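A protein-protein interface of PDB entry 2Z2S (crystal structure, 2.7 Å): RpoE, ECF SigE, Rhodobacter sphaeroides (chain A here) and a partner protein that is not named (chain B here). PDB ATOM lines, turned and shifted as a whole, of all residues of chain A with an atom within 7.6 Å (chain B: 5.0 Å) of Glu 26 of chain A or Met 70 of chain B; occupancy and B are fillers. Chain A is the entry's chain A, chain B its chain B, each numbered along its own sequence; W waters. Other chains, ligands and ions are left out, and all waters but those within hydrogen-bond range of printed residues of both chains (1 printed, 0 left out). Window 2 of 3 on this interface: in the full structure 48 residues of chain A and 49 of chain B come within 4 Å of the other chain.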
ATOM      1  N   ALA A  19      -1.806  -4.314  27.681  1.00  0.00           N
ATOM      2  CA  ALA A  19      -1.061  -5.534  27.933  1.00  0.00           C
ATOM      3  C   ALA A  19      -1.040  -6.343  26.659  1.00  0.00           C
ATOM      4  O   ALA A  19       0.002  -6.844  26.255  1.00  0.00           O
ATOM      5  CB  ALA A  19      -1.707  -6.331  29.059  1.00  0.00           C
ATOM      6  N   ILE A  20      -2.202  -6.453  26.027  1.00  0.00           N
ATOM      7  CA  ILE A  20      -2.368  -7.214  24.787  1.00  0.00           C
ATOM      8  C   ILE A  20      -1.658  -6.563  23.616  1.00  0.00           C
ATOM      9  O   ILE A  20      -1.044  -7.235  22.787  1.00  0.00           O
ATOM     10  CB  ILE A  20      -3.847  -7.349  24.414  1.00  0.00           C
ATOM     11  CG1 ILE A  20      -4.590  -8.117  25.497  1.00  0.00           C
ATOM     12  CG2 ILE A  20      -3.970  -8.051  23.098  1.00  0.00           C
ATOM     13  CD1 ILE A  20      -6.054  -8.280  25.226  1.00  0.00           C
ATOM     14  N   HIS A  23       2.325  -6.953  24.771  1.00  0.00           N
ATOM     15  CA  HIS A  23       2.932  -8.229  25.137  1.00  0.00           C
ATOM     16  C   HIS A  23       2.139  -9.483  24.788  1.00  0.00           C
ATOM     17  O   HIS A  23       2.518 -10.588  25.184  1.00  0.00           O
ATOM     18  CB  HIS A  23       3.243  -8.246  26.633  1.00  0.00           C
ATOM     19  CG  HIS A  23       4.008  -7.050  27.100  1.00  0.00           C
ATOM     20  ND1 HIS A  23       5.232  -6.699  26.572  1.00  0.00           N
ATOM     21  CD2 HIS A  23       3.717  -6.111  28.033  1.00  0.00           C
ATOM     22  CE1 HIS A  23       5.662  -5.596  27.159  1.00  0.00           C
ATOM     23  NE2 HIS A  23       4.762  -5.217  28.049  1.00  0.00           N
ATOM     24  N   ARG A  24       1.053  -9.332  24.041  1.00  0.00           N
ATOM     25  CA  ARG A  24       0.237 -10.487  23.699  1.00  0.00           C
ATOM     26  C   ARG A  24      -0.019 -11.280  24.982  1.00  0.00           C
ATOM     27  O   ARG A  24       0.081 -12.510  25.021  1.00  0.00           O
ATOM     28  CB  ARG A  24       0.955 -11.353  22.667  1.00  0.00           C
ATOM     29  CG  ARG A  24       1.401 -10.595  21.425  1.00  0.00           C
ATOM     30  CD  ARG A  24       1.829 -11.566  20.339  1.00  0.00           C
ATOM     31  NE  ARG A  24       2.498 -12.753  20.887  1.00  0.00           N
ATOM     32  CZ  ARG A  24       3.683 -12.755  21.500  1.00  0.00           C
ATOM     33  NH1 ARG A  24       4.361 -11.624  21.655  1.00  0.00           N
ATOM     34  NH2 ARG A  24       4.193 -13.895  21.964  1.00  0.00           N
ATOM     35  N   ASP A  25      -0.340 -10.530  26.031  1.00  0.00           N
ATOM     36  CA  ASP A  25      -0.616 -11.063  27.349  1.00  0.00           C
ATOM     37  C   ASP A  25      -1.933 -11.830  27.319  1.00  0.00           C
ATOM     38  O   ASP A  25      -2.991 -11.233  27.428  1.00  0.00           O
ATOM     39  CB  ASP A  25      -0.702  -9.895  28.330  1.00  0.00           C
ATOM     40  CG  ASP A  25      -0.814 -10.344  29.765  1.00  0.00           C
ATOM     41  OD1 ASP A  25      -1.425 -11.407  30.016  1.00  0.00           O
ATOM     42  OD2 ASP A  25      -0.307  -9.620  30.650  1.00  0.00           O
ATOM     43  N   GLU A  26      -1.868 -13.150  27.186  1.00  0.00           N
ATOM     44  CA  GLU A  26      -3.076 -13.978  27.124  1.00  0.00           C
ATOM     45  C   GLU A  26      -3.928 -13.978  28.384  1.00  0.00           C
ATOM     46  O   GLU A  26      -5.145 -14.158  28.309  1.00  0.00           O
ATOM     47  CB  GLU A  26      -2.714 -15.417  26.796  1.00  0.00           C
ATOM     48  CG  GLU A  26      -1.744 -15.545  25.658  1.00  0.00           C
ATOM     49  CD  GLU A  26      -1.527 -16.990  25.220  1.00  0.00           C
ATOM     50  OE1 GLU A  26      -1.220 -17.855  26.071  1.00  0.00           O
ATOM     51  OE2 GLU A  26      -1.652 -17.265  24.009  1.00  0.00           O
ATOM     52  N   ALA A  27      -3.298 -13.808  29.542  1.00  0.00           N
ATOM     53  CA  ALA A  27      -4.050 -13.784  30.792  1.00  0.00           C
ATOM     54  C   ALA A  27      -4.924 -12.545  30.734  1.00  0.00           C
ATOM     55  O   ALA A  27      -6.119 -12.603  31.011  1.00  0.00           O
ATOM     56  CB  ALA A  27      -3.104 -13.731  31.991  1.00  0.00           C
ATOM     57  N   ALA A  28      -4.319 -11.427  30.351  1.00  0.00           N
ATOM     58  CA  ALA A  28      -5.044 -10.172  30.227  1.00  0.00           C
ATOM     59  C   ALA A  28      -6.271 -10.363  29.342  1.00  0.00           C
ATOM     60  O   ALA A  28      -7.371  -9.867  29.653  1.00  0.00           O
ATOM     61  CB  ALA A  28      -4.142  -9.118  29.637  1.00  0.00           C
ATOM     62  N   PHE A  29      -6.075 -11.075  28.235  1.00  0.00           N
ATOM     63  CA  PHE A  29      -7.164 -11.338  27.311  1.00  0.00           C
ATOM     64  C   PHE A  29      -8.241 -12.142  28.023  1.00  0.00           C
ATOM     65  O   PHE A  29      -9.427 -11.859  27.874  1.00  0.00           O
ATOM     66  CB  PHE A  29      -6.670 -12.116  26.093  1.00  0.00           C
ATOM     67  CG  PHE A  29      -7.762 -12.492  25.149  1.00  0.00           C
ATOM     68  CD1 PHE A  29      -8.316 -11.534  24.309  1.00  0.00           C
ATOM     69  CD2 PHE A  29      -8.293 -13.777  25.159  1.00  0.00           C
ATOM     70  CE1 PHE A  29      -9.392 -11.840  23.495  1.00  0.00           C
ATOM     71  CE2 PHE A  29      -9.375 -14.097  24.347  1.00  0.00           C
ATOM     72  CZ  PHE A  29      -9.926 -13.126  23.514  1.00  0.00           C
ATOM     73  N   ALA A  30      -7.841 -13.152  28.795  1.00  0.00           N
ATOM     74  CA  ALA A  30      -8.835 -13.936  29.514  1.00  0.00           C
ATOM     75  C   ALA A  30      -9.563 -12.965  30.443  1.00  0.00           C
ATOM     76  O   ALA A  30     -10.801 -12.930  30.456  1.00  0.00           O
ATOM     77  CB  ALA A  30      -8.173 -15.056  30.305  1.00  0.00           C
ATOM     78  N   GLU A  31      -8.806 -12.161  31.197  1.00  0.00           N
ATOM     79  CA  GLU A  31      -9.425 -11.184  32.099  1.00  0.00           C
ATOM     80  C   GLU A  31     -10.511 -10.437  31.337  1.00  0.00           C
ATOM     81  O   GLU A  31     -11.647 -10.375  31.798  1.00  0.00           O
ATOM     82  CB  GLU A  31      -8.414 -10.169  32.631  1.00  0.00           C
ATOM     83  CG  GLU A  31      -7.402 -10.715  33.628  1.00  0.00           C
ATOM     84  CD  GLU A  31      -8.017 -11.258  34.905  1.00  0.00           C
ATOM     85  OE1 GLU A  31      -7.257 -11.489  35.894  1.00  0.00           O
ATOM     86  OE2 GLU A  31      -9.259 -11.452  34.896  1.00  0.00           O
ATOM     87  N   LEU A  32     -10.175  -9.877  30.173  1.00  0.00           N
ATOM     88  CA  LEU A  32     -11.171  -9.153  29.367  1.00  0.00           C
ATOM     89  C   LEU A  32     -12.355 -10.013  28.945  1.00  0.00           C
ATOM     90  O   LEU A  32     -13.508  -9.616  29.139  1.00  0.00           O
ATOM     91  CB  LEU A  32     -10.548  -8.538  28.102  1.00  0.00           C
ATOM     92  CG  LEU A  32      -9.769  -7.221  28.298  1.00  0.00           C
ATOM     93  CD1 LEU A  32      -8.970  -6.918  27.056  1.00  0.00           C
ATOM     94  CD2 LEU A  32     -10.703  -6.051  28.624  1.00  0.00           C
ATOM     95  N   PHE A  33     -12.065 -11.188  28.382  1.00  0.00           N
ATOM     96  CA  PHE A  33     -13.089 -12.092  27.889  1.00  0.00           C
ATOM     97  C   PHE A  33     -14.109 -12.495  28.925  1.00  0.00           C
ATOM     98  O   PHE A  33     -15.310 -12.488  28.661  1.00  0.00           O
ATOM     99  CB  PHE A  33     -12.457 -13.369  27.322  1.00  0.00           C
ATOM    100  CG  PHE A  33     -13.451 -14.310  26.665  1.00  0.00           C
ATOM    101  CD1 PHE A  33     -13.674 -14.250  25.286  1.00  0.00           C
ATOM    102  CD2 PHE A  33     -14.146 -15.275  27.426  1.00  0.00           C
ATOM    103  CE1 PHE A  33     -14.569 -15.138  24.666  1.00  0.00           C
ATOM    104  CE2 PHE A  33     -15.047 -16.171  26.823  1.00  0.00           C
ATOM    105  CZ  PHE A  33     -15.260 -16.105  25.440  1.00  0.00           C
ATOM    106  N   TRP A  66      -8.585  -9.067  20.178  1.00  0.00           N
ATOM    107  CA  TRP A  66      -7.194  -9.488  20.193  1.00  0.00           C
ATOM    108  C   TRP A  66      -6.414  -9.057  18.951  1.00  0.00           C
ATOM    109  O   TRP A  66      -5.319  -8.518  19.065  1.00  0.00           O
ATOM    110  CB  TRP A  66      -7.103 -11.010  20.352  1.00  0.00           C
ATOM    111  CG  TRP A  66      -5.688 -11.550  20.273  1.00  0.00           C
ATOM    112  CD1 TRP A  66      -4.999 -11.898  19.139  1.00  0.00           C
ATOM    113  CD2 TRP A  66      -4.784 -11.767  21.373  1.00  0.00           C
ATOM    114  NE1 TRP A  66      -3.726 -12.319  19.465  1.00  0.00           N
ATOM    115  CE2 TRP A  66      -3.564 -12.250  20.824  1.00  0.00           C
ATOM    116  CE3 TRP A  66      -4.885 -11.602  22.765  1.00  0.00           C
ATOM    117  CZ2 TRP A  66      -2.452 -12.567  21.623  1.00  0.00           C
ATOM    118  CZ3 TRP A  66      -3.782 -11.915  23.559  1.00  0.00           C
ATOM    119  CH2 TRP A  66      -2.581 -12.394  22.984  1.00  0.00           C
ATOM    120  N   SER B  65     -16.026 -21.912  26.300  1.00  0.00           N
ATOM    121  CA  SER B  65     -15.946 -20.841  25.327  1.00  0.00           C
ATOM    122  C   SER B  65     -14.641 -20.064  25.394  1.00  0.00           C
ATOM    123  O   SER B  65     -14.003 -19.840  24.360  1.00  0.00           O
ATOM    124  CB  SER B  65     -17.149 -19.922  25.465  1.00  0.00           C
ATOM    125  OG  SER B  65     -18.328 -20.619  25.077  1.00  0.00           O
ATOM    126  N   LEU B  66     -14.220 -19.669  26.592  1.00  0.00           N
ATOM    127  CA  LEU B  66     -12.965 -18.927  26.709  1.00  0.00           C
ATOM    128  C   LEU B  66     -11.799 -19.761  26.178  1.00  0.00           C
ATOM    129  O   LEU B  66     -11.030 -19.303  25.324  1.00  0.00           O
ATOM    130  CB  LEU B  66     -12.688 -18.534  28.170  1.00  0.00           C
ATOM    131  CG  LEU B  66     -11.235 -18.088  28.402  1.00  0.00           C
ATOM    132  CD1 LEU B  66     -10.886 -16.988  27.423  1.00  0.00           C
ATOM    133  CD2 LEU B  66     -11.027 -17.625  29.819  1.00  0.00           C
ATOM    134  N   ALA B  67     -11.686 -20.983  26.697  1.00  0.00           N
ATOM    135  CA  ALA B  67     -10.626 -21.920  26.319  1.00  0.00           C
ATOM    136  C   ALA B  67     -10.640 -22.152  24.806  1.00  0.00           C
ATOM    137  O   ALA B  67      -9.587 -22.226  24.147  1.00  0.00           O
ATOM    138  CB  ALA B  67     -10.818 -23.255  27.070  1.00  0.00           C
ATOM    139  N   SER B  68     -11.855 -22.259  24.276  1.00  0.00           N
ATOM    140  CA  SER B  68     -12.074 -22.469  22.861  1.00  0.00           C
ATOM    141  C   SER B  68     -11.479 -21.318  22.069  1.00  0.00           C
ATOM    142  O   SER B  68     -10.624 -21.519  21.215  1.00  0.00           O
ATOM    143  CB  SER B  68     -13.582 -22.569  22.589  1.00  0.00           C
ATOM    144  OG  SER B  68     -13.881 -22.660  21.202  1.00  0.00           O
ATOM    145  N   VAL B  69     -11.925 -20.106  22.368  1.00  0.00           N
ATOM    146  CA  VAL B  69     -11.440 -18.936  21.649  1.00  0.00           C
ATOM    147  C   VAL B  69      -9.937 -18.726  21.815  1.00  0.00           C
ATOM    148  O   VAL B  69      -9.261 -18.365  20.863  1.00  0.00           O
ATOM    149  CB  VAL B  69     -12.188 -17.649  22.096  1.00  0.00           C
ATOM    150  CG1 VAL B  69     -11.748 -16.464  21.250  1.00  0.00           C
ATOM    151  CG2 VAL B  69     -13.692 -17.849  21.985  1.00  0.00           C
ATOM    152  N   MET B  70      -9.415 -18.939  23.018  1.00  0.00           N
ATOM    153  CA  MET B  70      -7.987 -18.751  23.245  1.00  0.00           C
ATOM    154  C   MET B  70      -7.174 -19.707  22.376  1.00  0.00           C
ATOM    155  O   MET B  70      -6.043 -19.421  21.976  1.00  0.00           O
ATOM    156  CB  MET B  70      -7.641 -18.981  24.718  1.00  0.00           C
ATOM    157  CG  MET B  70      -7.587 -17.712  25.556  1.00  0.00           C
ATOM    158  SD  MET B  70      -6.548 -17.972  27.158  1.00  0.00           S
ATOM    159  CE  MET B  70      -4.792 -18.152  26.378  1.00  0.00           C
ATOM    160  N   ALA B  71      -7.756 -20.855  22.078  1.00  0.00           N
ATOM    161  CA  ALA B  71      -7.054 -21.835  21.268  1.00  0.00           C
ATOM    162  C   ALA B  71      -6.825 -21.324  19.858  1.00  0.00           C
ATOM    163  O   ALA B  71      -5.775 -21.556  19.278  1.00  0.00           O
ATOM    164  CB  ALA B  71      -7.831 -23.134  21.232  1.00  0.00           C
ATOM    165  N   GLN B  72      -7.812 -20.625  19.311  1.00  0.00           N
ATOM    166  CA  GLN B  72      -7.717 -20.101  17.955  1.00  0.00           C
ATOM    167  C   GLN B  72      -7.227 -18.656  17.829  1.00  0.00           C
ATOM    168  O   GLN B  72      -7.510 -17.995  16.836  1.00  0.00           O
ATOM    169  CB  GLN B  72      -9.080 -20.230  17.267  1.00  0.00           C
ATOM    170  CG  GLN B  72      -9.362 -21.604  16.725  1.00  0.00           C
ATOM    171  CD  GLN B  72      -8.352 -21.994  15.681  1.00  0.00           C
ATOM    172  OE1 GLN B  72      -7.468 -22.817  15.936  1.00  0.00           O
ATOM    173  NE2 GLN B  72      -8.457 -21.385  14.495  1.00  0.00           N
ATOM    174  N   LEU B  73      -6.496 -18.159  18.820  1.00  0.00           N
ATOM    175  CA  LEU B  73      -5.999 -16.782  18.769  1.00  0.00           C
ATOM    176  C   LEU B  73      -4.585 -16.761  18.244  1.00  0.00           C
ATOM    177  O   LEU B  73      -3.775 -17.605  18.629  1.00  0.00           O
ATOM    178  CB  LEU B  73      -5.988 -16.150  20.153  1.00  0.00           C
ATOM    179  CG  LEU B  73      -7.320 -15.845  20.806  1.00  0.00           C
ATOM    180  CD1 LEU B  73      -7.074 -15.114  22.118  1.00  0.00           C
ATOM    181  CD2 LEU B  73      -8.144 -14.993  19.871  1.00  0.00           C
HETATM  182  O   HOH W   1      -2.973 -18.815  22.606  1.00  0.00           O
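Water W1 bridges OE2 of Glu 26 of chain A (2.5 Å) and O of Met 70 of chain B (3.2 Å).
Arg 24 of chain A touches none of the printed residues of chain B.
Of chain B, only Met 70 (3.5 Å) comes within 4 Å of Glu 26 of chain A.
Of the printed residues of chain B, Phe 29 of chain A touches Leu 73.
Of the printed residues of chain B, Ala 30 of chain A touches Leu 66 (3.9 Å).
Leu 32 of chain A touches none of the printed residues of chain B.
Of the printed residues of chain A, Leu 66 of chain B touches Ala 30 and Phe 33.
Printed residues of chain A within 4 Å of Val 69 of chain B: Phe 33.
Of the printed residues of chain A, Met 70 of chain B touches Glu 26 (3.5 Å).
The nearest printed residue of chain B that does not touch Glu 26 of chain A is Leu 73 of chain B (5.8 Å).
Hydrophobic or aromatic side chains of chain B within 4 Å of the printed part of chain A: Leu 66, Val 69, Met 70 and Leu 73.
Of the 14 printed residues of chain A, 4 touch a printed residue of chain B.
Printed residues of chain A that touch a printed residue of chain B: Glu 26, Phe 29, Ala 30 and Phe 33.
Hydrophobic or aromatic side chains of chain A within 4 Å of the printed part of chain B: Phe 29, Ala 30 and Phe 33.
Among the printed residues, 5 pairs touch across the chains.
Among the printed residues, merely in contact across the chains: Phe 29 of chain A with Leu 73 of chain B, Phe 33 of chain A with Leu 66 of chain B, Glu 26 of chain A with Met 70 of chain B, Ala 30 of chain A with Leu 66 of chain B and Phe 33 of chain A with Val 69 of chain B.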
